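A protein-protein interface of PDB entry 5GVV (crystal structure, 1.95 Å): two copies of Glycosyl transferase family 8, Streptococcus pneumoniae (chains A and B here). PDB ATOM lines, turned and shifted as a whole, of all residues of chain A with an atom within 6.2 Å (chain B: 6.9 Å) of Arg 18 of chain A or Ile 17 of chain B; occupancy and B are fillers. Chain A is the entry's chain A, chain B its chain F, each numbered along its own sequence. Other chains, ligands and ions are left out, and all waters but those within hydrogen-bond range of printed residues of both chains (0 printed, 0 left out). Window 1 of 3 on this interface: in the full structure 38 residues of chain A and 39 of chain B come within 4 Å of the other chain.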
ATOM      1  N   TYR A  14     -15.281  27.046   9.699  1.00  0.00           N
ATOM      2  CA  TYR A  14     -16.195  27.984  10.345  1.00  0.00           C
ATOM      3  C   TYR A  14     -16.902  27.344  11.538  1.00  0.00           C
ATOM      4  O   TYR A  14     -17.221  28.018  12.514  1.00  0.00           O
ATOM      5  CB  TYR A  14     -17.230  28.448   9.315  1.00  0.00           C
ATOM      6  CG  TYR A  14     -18.108  29.620   9.716  1.00  0.00           C
ATOM      7  CD1 TYR A  14     -17.718  30.529  10.693  1.00  0.00           C
ATOM      8  CD2 TYR A  14     -19.331  29.823   9.092  1.00  0.00           C
ATOM      9  CE1 TYR A  14     -18.542  31.606  11.042  1.00  0.00           C
ATOM     10  CE2 TYR A  14     -20.151  30.881   9.431  1.00  0.00           C
ATOM     11  CZ  TYR A  14     -19.755  31.767  10.403  1.00  0.00           C
ATOM     12  OH  TYR A  14     -20.591  32.819  10.716  1.00  0.00           O
ATOM     13  N   ALA A  15     -17.155  26.042  11.457  1.00  0.00           N
ATOM     14  CA  ALA A  15     -17.853  25.344  12.531  1.00  0.00           C
ATOM     15  C   ALA A  15     -17.003  25.322  13.794  1.00  0.00           C
ATOM     16  O   ALA A  15     -17.520  25.143  14.894  1.00  0.00           O
ATOM     17  CB  ALA A  15     -18.215  23.930  12.103  1.00  0.00           C
ATOM     18  N   TYR A  16     -15.697  25.505  13.619  1.00  0.00           N
ATOM     19  CA  TYR A  16     -14.751  25.506  14.727  1.00  0.00           C
ATOM     20  C   TYR A  16     -14.354  26.942  15.087  1.00  0.00           C
ATOM     21  O   TYR A  16     -13.381  27.160  15.812  1.00  0.00           O
ATOM     22  CB  TYR A  16     -13.503  24.719  14.311  1.00  0.00           C
ATOM     23  CG  TYR A  16     -12.955  23.744  15.334  1.00  0.00           C
ATOM     24  CD1 TYR A  16     -13.678  22.621  15.722  1.00  0.00           C
ATOM     25  CD2 TYR A  16     -11.690  23.924  15.880  1.00  0.00           C
ATOM     26  CE1 TYR A  16     -13.161  21.717  16.648  1.00  0.00           C
ATOM     27  CE2 TYR A  16     -11.168  23.028  16.807  1.00  0.00           C
ATOM     28  CZ  TYR A  16     -11.908  21.930  17.184  1.00  0.00           C
ATOM     29  OH  TYR A  16     -11.385  21.039  18.097  1.00  0.00           O
ATOM     30  N   ILE A  17     -15.104  27.927  14.596  1.00  0.00           N
ATOM     31  CA  ILE A  17     -14.717  29.327  14.795  1.00  0.00           C
ATOM     32  C   ILE A  17     -14.578  29.740  16.272  1.00  0.00           C
ATOM     33  O   ILE A  17     -13.707  30.557  16.605  1.00  0.00           O
ATOM     34  CB  ILE A  17     -15.655  30.303  14.031  1.00  0.00           C
ATOM     35  CG1 ILE A  17     -15.010  31.688  13.907  1.00  0.00           C
ATOM     36  CG2 ILE A  17     -17.023  30.388  14.708  1.00  0.00           C
ATOM     37  CD1 ILE A  17     -13.792  31.720  12.980  1.00  0.00           C
ATOM     38  N   ARG A  18     -15.407  29.169  17.152  1.00  0.00           N
ATOM     39  CA  ARG A  18     -15.353  29.508  18.578  1.00  0.00           C
ATOM     40  C   ARG A  18     -14.051  29.023  19.212  1.00  0.00           C
ATOM     41  O   ARG A  18     -13.527  29.651  20.136  1.00  0.00           O
ATOM     42  CB  ARG A  18     -16.555  28.932  19.345  1.00  0.00           C
ATOM     43  CG  ARG A  18     -17.863  29.695  19.136  1.00  0.00           C
ATOM     44  CD  ARG A  18     -19.011  29.101  19.947  1.00  0.00           C
ATOM     45  NE  ARG A  18     -18.830  29.293  21.384  1.00  0.00           N
ATOM     46  CZ  ARG A  18     -18.657  28.300  22.251  1.00  0.00           C
ATOM     47  NH1 ARG A  18     -18.646  27.045  21.822  1.00  0.00           N
ATOM     48  NH2 ARG A  18     -18.495  28.558  23.544  1.00  0.00           N
ATOM     49  N   GLN A  19     -13.531  27.905  18.709  1.00  0.00           N
ATOM     50  CA  GLN A  19     -12.275  27.347  19.204  1.00  0.00           C
ATOM     51  C   GLN A  19     -11.087  28.087  18.593  1.00  0.00           C
ATOM     52  O   GLN A  19     -10.129  28.427  19.291  1.00  0.00           O
ATOM     53  CB  GLN A  19     -12.187  25.852  18.874  1.00  0.00           C
ATOM     54  CG  GLN A  19     -13.185  24.965  19.633  1.00  0.00           C
ATOM     55  CD  GLN A  19     -14.637  25.221  19.248  1.00  0.00           C
ATOM     56  OE1 GLN A  19     -14.967  25.337  18.067  1.00  0.00           O
ATOM     57  NE2 GLN A  19     -15.506  25.328  20.245  1.00  0.00           N
ATOM     58  N   ILE A  20     -11.153  28.335  17.287  1.00  0.00           N
ATOM     59  CA  ILE A  20     -10.108  29.091  16.608  1.00  0.00           C
ATOM     60  C   ILE A  20      -9.948  30.463  17.245  1.00  0.00           C
ATOM     61  O   ILE A  20      -8.831  30.883  17.546  1.00  0.00           O
ATOM     62  CB  ILE A  20     -10.419  29.274  15.108  1.00  0.00           C
ATOM     63  CG1 ILE A  20     -10.539  27.918  14.415  1.00  0.00           C
ATOM     64  CG2 ILE A  20      -9.350  30.143  14.425  1.00  0.00           C
ATOM     65  CD1 ILE A  20     -11.102  28.008  13.000  1.00  0.00           C
ATOM     66  N   GLU A  21     -11.060  31.161  17.461  1.00  0.00           N
ATOM     67  CA  GLU A  21     -10.996  32.518  17.994  1.00  0.00           C
ATOM     68  C   GLU A  21     -10.494  32.547  19.431  1.00  0.00           C
ATOM     69  O   GLU A  21      -9.733  33.441  19.804  1.00  0.00           O
ATOM     70  CB  GLU A  21     -12.357  33.226  17.886  1.00  0.00           C
ATOM     71  CG  GLU A  21     -12.270  34.720  18.188  1.00  0.00           C
ATOM     72  CD  GLU A  21     -13.550  35.476  17.879  1.00  0.00           C
ATOM     73  OE1 GLU A  21     -14.422  34.926  17.166  1.00  0.00           O
ATOM     74  OE2 GLU A  21     -13.678  36.626  18.352  1.00  0.00           O
ATOM     75  N   THR A  22     -10.928  31.576  20.234  1.00  0.00           N
ATOM     76  CA  THR A  22     -10.447  31.438  21.607  1.00  0.00           C
ATOM     77  C   THR A  22      -8.938  31.182  21.664  1.00  0.00           C
ATOM     78  O   THR A  22      -8.232  31.773  22.479  1.00  0.00           O
ATOM     79  CB  THR A  22     -11.183  30.310  22.338  1.00  0.00           C
ATOM     80  OG1 THR A  22     -12.573  30.648  22.448  1.00  0.00           O
ATOM     81  CG2 THR A  22     -10.615  30.115  23.739  1.00  0.00           C
ATOM     82  N   ALA A  23      -8.443  30.301  20.801  1.00  0.00           N
ATOM     83  CA  ALA A  23      -7.009  30.005  20.773  1.00  0.00           C
ATOM     84  C   ALA A  23      -6.219  31.242  20.354  1.00  0.00           C
ATOM     85  O   ALA A  23      -5.173  31.544  20.933  1.00  0.00           O
ATOM     86  CB  ALA A  23      -6.726  28.854  19.839  1.00  0.00           C
ATOM     87  N   TRP A 235     -15.020  22.718  26.143  1.00  0.00           N
ATOM     88  CA  TRP A 235     -16.142  23.535  25.703  1.00  0.00           C
ATOM     89  C   TRP A 235     -17.446  22.750  25.567  1.00  0.00           C
ATOM     90  O   TRP A 235     -18.503  23.334  25.318  1.00  0.00           O
ATOM     91  CB  TRP A 235     -15.818  24.261  24.396  1.00  0.00           C
ATOM     92  CG  TRP A 235     -15.498  23.374  23.223  1.00  0.00           C
ATOM     93  CD1 TRP A 235     -16.390  22.743  22.399  1.00  0.00           C
ATOM     94  CD2 TRP A 235     -14.192  23.057  22.721  1.00  0.00           C
ATOM     95  NE1 TRP A 235     -15.716  22.044  21.423  1.00  0.00           N
ATOM     96  CE2 TRP A 235     -14.365  22.222  21.594  1.00  0.00           C
ATOM     97  CE3 TRP A 235     -12.893  23.398  23.105  1.00  0.00           C
ATOM     98  CZ2 TRP A 235     -13.289  21.724  20.856  1.00  0.00           C
ATOM     99  CZ3 TRP A 235     -11.818  22.896  22.372  1.00  0.00           C
ATOM    100  CH2 TRP A 235     -12.027  22.067  21.263  1.00  0.00           C
ATOM    101  N   TRP A 247     -10.039  27.365  29.597  1.00  0.00           N
ATOM    102  CA  TRP A 247     -10.533  27.571  28.239  1.00  0.00           C
ATOM    103  C   TRP A 247     -11.646  28.598  28.230  1.00  0.00           C
ATOM    104  O   TRP A 247     -11.678  29.474  27.366  1.00  0.00           O
ATOM    105  CB  TRP A 247     -11.039  26.267  27.605  1.00  0.00           C
ATOM    106  CG  TRP A 247     -11.393  26.437  26.132  1.00  0.00           C
ATOM    107  CD1 TRP A 247     -10.559  26.251  25.056  1.00  0.00           C
ATOM    108  CD2 TRP A 247     -12.658  26.854  25.590  1.00  0.00           C
ATOM    109  NE1 TRP A 247     -11.232  26.520  23.885  1.00  0.00           N
ATOM    110  CE2 TRP A 247     -12.522  26.885  24.183  1.00  0.00           C
ATOM    111  CE3 TRP A 247     -13.897  27.190  26.152  1.00  0.00           C
ATOM    112  CZ2 TRP A 247     -13.578  27.250  23.333  1.00  0.00           C
ATOM    113  CZ3 TRP A 247     -14.944  27.547  25.310  1.00  0.00           C
ATOM    114  CH2 TRP A 247     -14.776  27.578  23.914  1.00  0.00           C
ATOM    115  N   TRP A 248     -12.563  28.483  29.185  1.00  0.00           N
ATOM    116  CA  TRP A 248     -13.693  29.396  29.252  1.00  0.00           C
ATOM    117  C   TRP A 248     -13.260  30.825  29.562  1.00  0.00           C
ATOM    118  O   TRP A 248     -13.842  31.783  29.043  1.00  0.00           O
ATOM    119  CB  TRP A 248     -14.732  28.880  30.252  1.00  0.00           C
ATOM    120  CG  TRP A 248     -15.512  27.763  29.651  1.00  0.00           C
ATOM    121  CD1 TRP A 248     -15.326  26.426  29.850  1.00  0.00           C
ATOM    122  CD2 TRP A 248     -16.566  27.882  28.690  1.00  0.00           C
ATOM    123  NE1 TRP A 248     -16.217  25.707  29.093  1.00  0.00           N
ATOM    124  CE2 TRP A 248     -16.993  26.580  28.370  1.00  0.00           C
ATOM    125  CE3 TRP A 248     -17.201  28.969  28.080  1.00  0.00           C
ATOM    126  CZ2 TRP A 248     -18.024  26.332  27.462  1.00  0.00           C
ATOM    127  CZ3 TRP A 248     -18.228  28.722  27.174  1.00  0.00           C
ATOM    128  CH2 TRP A 248     -18.628  27.416  26.876  1.00  0.00           C
ATOM    129  N   SER A 251     -12.324  32.141  26.244  1.00  0.00           N
ATOM    130  CA  SER A 251     -13.476  32.190  25.341  1.00  0.00           C
ATOM    131  C   SER A 251     -14.377  33.393  25.636  1.00  0.00           C
ATOM    132  O   SER A 251     -14.889  34.045  24.715  1.00  0.00           O
ATOM    133  CB  SER A 251     -14.293  30.899  25.437  1.00  0.00           C
ATOM    134  OG  SER A 251     -15.459  30.978  24.633  1.00  0.00           O
ATOM    135  N   GLY B  12     -33.006  28.161  22.247  1.00  0.00           N
ATOM    136  CA  GLY B  12     -32.083  27.651  21.255  1.00  0.00           C
ATOM    137  C   GLY B  12     -31.053  26.714  21.839  1.00  0.00           C
ATOM    138  O   GLY B  12     -30.888  26.637  23.064  1.00  0.00           O
ATOM    139  N   ASP B  13     -30.349  25.999  20.967  1.00  0.00           N
ATOM    140  CA  ASP B  13     -29.328  25.066  21.426  1.00  0.00           C
ATOM    141  C   ASP B  13     -27.920  25.636  21.291  1.00  0.00           C
ATOM    142  O   ASP B  13     -27.721  26.683  20.665  1.00  0.00           O
ATOM    143  CB  ASP B  13     -29.453  23.721  20.700  1.00  0.00           C
ATOM    144  CG  ASP B  13     -29.323  23.846  19.195  1.00  0.00           C
ATOM    145  OD1 ASP B  13     -29.642  24.920  18.637  1.00  0.00           O
ATOM    146  OD2 ASP B  13     -28.914  22.851  18.561  1.00  0.00           O
ATOM    147  N   TYR B  14     -26.953  24.932  21.883  1.00  0.00           N
ATOM    148  CA  TYR B  14     -25.550  25.343  21.915  1.00  0.00           C
ATOM    149  C   TYR B  14     -24.978  25.548  20.510  1.00  0.00           C
ATOM    150  O   TYR B  14     -24.111  26.398  20.307  1.00  0.00           O
ATOM    151  CB  TYR B  14     -24.744  24.278  22.677  1.00  0.00           C
ATOM    152  CG  TYR B  14     -23.319  24.643  23.061  1.00  0.00           C
ATOM    153  CD1 TYR B  14     -22.907  25.964  23.179  1.00  0.00           C
ATOM    154  CD2 TYR B  14     -22.383  23.646  23.310  1.00  0.00           C
ATOM    155  CE1 TYR B  14     -21.595  26.278  23.533  1.00  0.00           C
ATOM    156  CE2 TYR B  14     -21.079  23.950  23.664  1.00  0.00           C
ATOM    157  CZ  TYR B  14     -20.692  25.265  23.779  1.00  0.00           C
ATOM    158  OH  TYR B  14     -19.385  25.567  24.127  1.00  0.00           O
ATOM    159  N   ALA B  15     -25.459  24.776  19.536  1.00  0.00           N
ATOM    160  CA  ALA B  15     -24.990  24.933  18.159  1.00  0.00           C
ATOM    161  C   ALA B  15     -25.344  26.310  17.618  1.00  0.00           C
ATOM    162  O   ALA B  15     -24.717  26.800  16.674  1.00  0.00           O
ATOM    163  CB  ALA B  15     -25.580  23.850  17.268  1.00  0.00           C
ATOM    164  N   TYR B  16     -26.355  26.931  18.221  1.00  0.00           N
ATOM    165  CA  TYR B  16     -26.851  28.227  17.778  1.00  0.00           C
ATOM    166  C   TYR B  16     -26.368  29.347  18.700  1.00  0.00           C
ATOM    167  O   TYR B  16     -26.902  30.459  18.671  1.00  0.00           O
ATOM    168  CB  TYR B  16     -28.381  28.197  17.768  1.00  0.00           C
ATOM    169  CG  TYR B  16     -29.042  28.779  16.529  1.00  0.00           C
ATOM    170  CD1 TYR B  16     -28.860  28.203  15.275  1.00  0.00           C
ATOM    171  CD2 TYR B  16     -29.882  29.882  16.625  1.00  0.00           C
ATOM    172  CE1 TYR B  16     -29.486  28.729  14.144  1.00  0.00           C
ATOM    173  CE2 TYR B  16     -30.505  30.417  15.502  1.00  0.00           C
ATOM    174  CZ  TYR B  16     -30.307  29.834  14.271  1.00  0.00           C
ATOM    175  OH  TYR B  16     -30.936  30.364  13.164  1.00  0.00           O
ATOM    176  N   ILE B  17     -25.349  29.064  19.507  1.00  0.00           N
ATOM    177  CA  ILE B  17     -24.918  30.012  20.536  1.00  0.00           C
ATOM    178  C   ILE B  17     -24.408  31.348  19.960  1.00  0.00           C
ATOM    179  O   ILE B  17     -24.571  32.404  20.587  1.00  0.00           O
ATOM    180  CB  ILE B  17     -23.875  29.372  21.490  1.00  0.00           C
ATOM    181  CG1 ILE B  17     -23.758  30.170  22.790  1.00  0.00           C
ATOM    182  CG2 ILE B  17     -22.514  29.233  20.795  1.00  0.00           C
ATOM    183  CD1 ILE B  17     -25.074  30.296  23.559  1.00  0.00           C
ATOM    184  N   ARG B  18     -23.820  31.314  18.764  1.00  0.00           N
ATOM    185  CA  ARG B  18     -23.333  32.543  18.140  1.00  0.00           C
ATOM    186  C   ARG B  18     -24.500  33.446  17.745  1.00  0.00           C
ATOM    187  O   ARG B  18     -24.405  34.676  17.821  1.00  0.00           O
ATOM    188  CB  ARG B  18     -22.447  32.235  16.928  1.00  0.00           C
ATOM    189  CG  ARG B  18     -21.122  31.577  17.295  1.00  0.00           C
ATOM    190  CD  ARG B  18     -20.247  31.353  16.069  1.00  0.00           C
ATOM    191  NE  ARG B  18     -19.845  32.611  15.444  1.00  0.00           N
ATOM    192  CZ  ARG B  18     -20.271  33.025  14.253  1.00  0.00           C
ATOM    193  NH1 ARG B  18     -21.104  32.274  13.544  1.00  0.00           N
ATOM    194  NH2 ARG B  18     -19.853  34.187  13.760  1.00  0.00           N
ATOM    195  N   GLN B  19     -25.610  32.831  17.352  1.00  0.00           N
ATOM    196  CA  GLN B  19     -26.799  33.584  16.952  1.00  0.00           C
ATOM    197  C   GLN B  19     -27.551  34.080  18.180  1.00  0.00           C
ATOM    198  O   GLN B  19     -28.023  35.216  18.218  1.00  0.00           O
ATOM    199  CB  GLN B  19     -27.716  32.718  16.085  1.00  0.00           C
ATOM    200  CG  GLN B  19     -27.143  32.379  14.701  1.00  0.00           C
ATOM    201  CD  GLN B  19     -25.896  31.506  14.770  1.00  0.00           C
ATOM    202  OE1 GLN B  19     -25.772  30.652  15.648  1.00  0.00           O
ATOM    203  NE2 GLN B  19     -24.960  31.732  13.854  1.00  0.00           N
ATOM    204  N   ILE B  20     -27.668  33.223  19.186  1.00  0.00           N
ATOM    205  CA  ILE B  20     -28.314  33.608  20.432  1.00  0.00           C
ATOM    206  C   ILE B  20     -27.599  34.788  21.089  1.00  0.00           C
ATOM    207  O   ILE B  20     -28.242  35.755  21.505  1.00  0.00           O
ATOM    208  CB  ILE B  20     -28.365  32.426  21.423  1.00  0.00           C
ATOM    209  CG1 ILE B  20     -29.224  31.294  20.855  1.00  0.00           C
ATOM    210  CG2 ILE B  20     -28.901  32.879  22.767  1.00  0.00           C
ATOM    211  CD1 ILE B  20     -29.092  29.978  21.614  1.00  0.00           C
ATOM    212  N   GLU B  21     -26.275  34.717  21.185  1.00  0.00           N
ATOM    213  CA  GLU B  21     -25.536  35.764  21.878  1.00  0.00           C
ATOM    214  C   GLU B  21     -25.581  37.081  21.112  1.00  0.00           C
ATOM    215  O   GLU B  21     -25.650  38.155  21.716  1.00  0.00           O
ATOM    216  CB  GLU B  21     -24.088  35.337  22.158  1.00  0.00           C
ATOM    217  CG  GLU B  21     -23.321  36.362  23.001  1.00  0.00           C
ATOM    218  CD  GLU B  21     -21.961  35.871  23.462  1.00  0.00           C
ATOM    219  OE1 GLU B  21     -21.702  34.649  23.383  1.00  0.00           O
ATOM    220  OE2 GLU B  21     -21.150  36.715  23.905  1.00  0.00           O
ATOM    221  N   THR B  22     -25.535  36.998  19.783  1.00  0.00           N
ATOM    222  CA  THR B  22     -25.652  38.181  18.936  1.00  0.00           C
ATOM    223  C   THR B  22     -27.015  38.842  19.143  1.00  0.00           C
ATOM    224  O   THR B  22     -27.103  40.048  19.378  1.00  0.00           O
ATOM    225  CB  THR B  22     -25.448  37.819  17.455  1.00  0.00           C
ATOM    226  OG1 THR B  22     -24.137  37.259  17.286  1.00  0.00           O
ATOM    227  CG2 THR B  22     -25.579  39.050  16.564  1.00  0.00           C
ATOM    228  N   ALA B  23     -28.077  38.051  19.065  1.00  0.00           N
ATOM    229  CA  ALA B  23     -29.425  38.570  19.288  1.00  0.00           C
ATOM    230  C   ALA B  23     -29.543  39.243  20.657  1.00  0.00           C
ATOM    231  O   ALA B  23     -30.075  40.356  20.769  1.00  0.00           O
ATOM    232  CB  ALA B  23     -30.434  37.461  19.150  1.00  0.00           C
ATOM    233  N   LEU B  38     -33.599  31.907  29.031  1.00  0.00           N
ATOM    234  CA  LEU B  38     -33.088  31.198  27.862  1.00  0.00           C
ATOM    235  C   LEU B  38     -33.389  29.709  27.938  1.00  0.00           C
ATOM    236  O   LEU B  38     -32.783  28.975  28.729  1.00  0.00           O
ATOM    237  CB  LEU B  38     -31.584  31.448  27.683  1.00  0.00           C
ATOM    238  CG  LEU B  38     -30.833  30.688  26.587  1.00  0.00           C
ATOM    239  CD1 LEU B  38     -31.526  30.818  25.241  1.00  0.00           C
ATOM    240  CD2 LEU B  38     -29.422  31.221  26.493  1.00  0.00           C
ATOM    241  N   ILE B  43     -26.528  24.214  26.626  1.00  0.00           N
ATOM    242  CA  ILE B  43     -25.584  25.327  26.770  1.00  0.00           C
ATOM    243  C   ILE B  43     -24.780  25.223  28.081  1.00  0.00           C
ATOM    244  O   ILE B  43     -25.357  25.087  29.165  1.00  0.00           O
ATOM    245  CB  ILE B  43     -26.287  26.697  26.648  1.00  0.00           C
ATOM    246  CG1 ILE B  43     -27.019  26.799  25.311  1.00  0.00           C
ATOM    247  CG2 ILE B  43     -25.292  27.844  26.763  1.00  0.00           C
ATOM    248  CD1 ILE B  43     -27.876  28.049  25.182  1.00  0.00           C
ATOM    249  N   PRO B  44     -23.439  25.272  27.977  1.00  0.00           N
ATOM    250  CA  PRO B  44     -22.541  25.156  29.137  1.00  0.00           C
ATOM    251  C   PRO B  44     -22.772  26.224  30.209  1.00  0.00           C
ATOM    252  O   PRO B  44     -23.082  27.372  29.880  1.00  0.00           O
ATOM    253  CB  PRO B  44     -21.159  25.346  28.516  1.00  0.00           C
ATOM    254  CG  PRO B  44     -21.308  24.814  27.122  1.00  0.00           C
ATOM    255  CD  PRO B  44     -22.686  25.288  26.707  1.00  0.00           C
ATOM    256  N   TRP B  47     -20.846  29.794  30.227  1.00  0.00           N
ATOM    257  CA  TRP B  47     -21.371  30.856  29.382  1.00  0.00           C
ATOM    258  C   TRP B  47     -22.445  31.611  30.151  1.00  0.00           C
ATOM    259  O   TRP B  47     -22.444  32.841  30.178  1.00  0.00           O
ATOM    260  CB  TRP B  47     -21.938  30.263  28.084  1.00  0.00           C
ATOM    261  CG  TRP B  47     -22.451  31.279  27.099  1.00  0.00           C
ATOM    262  CD1 TRP B  47     -21.747  31.885  26.088  1.00  0.00           C
ATOM    263  CD2 TRP B  47     -23.783  31.797  27.021  1.00  0.00           C
ATOM    264  NE1 TRP B  47     -22.562  32.750  25.399  1.00  0.00           N
ATOM    265  CE2 TRP B  47     -23.818  32.715  25.955  1.00  0.00           C
ATOM    266  CE3 TRP B  47     -24.952  31.573  27.756  1.00  0.00           C
ATOM    267  CZ2 TRP B  47     -24.979  33.411  25.600  1.00  0.00           C
ATOM    268  CZ3 TRP B  47     -26.105  32.271  27.406  1.00  0.00           C
ATOM    269  CH2 TRP B  47     -26.107  33.177  26.339  1.00  0.00           C
ATOM    270  N   PHE B  48     -23.350  30.871  30.790  1.00  0.00           N
ATOM    271  CA  PHE B  48     -24.416  31.485  31.573  1.00  0.00           C
ATOM    272  C   PHE B  48     -23.870  32.327  32.717  1.00  0.00           C
ATOM    273  O   PHE B  48     -24.369  33.423  32.970  1.00  0.00           O
ATOM    274  CB  PHE B  48     -25.359  30.418  32.134  1.00  0.00           C
ATOM    275  CG  PHE B  48     -26.543  30.132  31.259  1.00  0.00           C
ATOM    276  CD1 PHE B  48     -27.635  30.989  31.249  1.00  0.00           C
ATOM    277  CD2 PHE B  48     -26.572  29.001  30.456  1.00  0.00           C
ATOM    278  CE1 PHE B  48     -28.734  30.736  30.435  1.00  0.00           C
ATOM    279  CE2 PHE B  48     -27.668  28.731  29.647  1.00  0.00           C
ATOM    280  CZ  PHE B  48     -28.751  29.599  29.637  1.00  0.00           C
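The side-chain hydroxyl (OH) of Tyr 14 of chain A is in hydrogen-bond range of the guanidinium group (NH1) of Arg 18 of chain B (2.9 Å). The guanidinium group (NH1) of Arg 18 of chain A sits at hydrogen-bond distance from the side-chain hydroxyl (OH) of Tyr 14 of chain B, at 2.8 Å. The backbone carbonyl oxygen of Trp 235 of chain A sits at hydrogen-bond distance from the side-chain hydroxyl of Tyr 14 of chain B (2.7 Å).
The backbone carbonyl oxygen (O) of Arg 18 of chain A is in hydrogen-bond range of the side-chain hydroxyl (OG1) of Thr 22 of chain A (2.7 Å). The side-chain amide nitrogen (NE2) of Gln 19 of chain A sits close to the indole nitrogen (NE1) of Trp 235 of chain A (3.5 Å). OG1 of Thr 22 of chain B lies within hydrogen-bond range of O of Arg 18 of chain B (2.7 Å).
Of chain B, only Tyr 14 (2.8 Å) and Ile 17 (3.6 Å) come within 4 Å of Arg 18 of chain A. Of chain A, only Arg 18 comes within 4 Å of Ile 17 of chain B. Of the printed residues of chain B, Ile 17 of chain A touches Arg 18. Of the printed residues of chain A, Pro 44 of chain B touches Trp 235 (3.6 Å) and Trp 248 (3.5 Å). Of the printed residues of chain A, Tyr 14 of chain B touches Arg 18 (2.8 Å), Trp 235 (2.7 Å) and Trp 248 (3.4 Å). Of the printed residues of chain B, Trp 235 of chain A touches Tyr 14 and Pro 44. Of the printed residues of chain B, Trp 248 of chain A touches Tyr 14 (3.4 Å) and Pro 44 (3.5 Å). Gln 19 of chain A touches none of the printed residues of chain B.
CG2 of Ile 17 of chain A touches CD of Arg 18 of chain B, 3.6 Å away. CD of Arg 18 of chain A touches CG2 of Ile 17 of chain B (3.6 Å). Trp 235 of chain A touches Pro 44 of chain B. Trp 248 of chain A touches Tyr 14 of chain B. Trp 248 of chain A touches Pro 44 of chain B.
Of the 17 printed residues of chain B, 4 touch a printed residue of chain A. Printed residues of chain B that touch a printed residue of chain A: Tyr 14, Ile 17, Arg 18 and Pro 44. Hydrophobic or aromatic side chains of chain B that line the printed part of chain A: Tyr 14, Ile 17 and Pro 44. Along chain B the printed residues that touch a printed residue of chain A span positions 14 to 44. Printed residues of chain A that touch a printed residue of chain B: Tyr 14, Ile 17, Arg 18, Trp 235 and Trp 248. Hydrophobic or aromatic side chains of chain A that line the printed part of chain B: Tyr 14, Ile 17, Trp 235 and Trp 248. Among the printed residues, 8 pairs touch across the chains. Among the printed residues, no Asp or Glu carboxylate lies within 4 Å of a Lys or Arg side-chain nitrogen of the other chain.
Tyr 14 of chain A touches Arg 18 of chain B, and with the chains exchanged Arg 18 of chain A touches Tyr 14 of chain B. Ile 17 of chain A touches Arg 18 of chain B, and with the chains exchanged Arg 18 of chain A touches Ile 17 of chain B. Of the 8 pairs that touch across the chains among the printed residues, 4 have their exchanged pair printed and touching as well.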
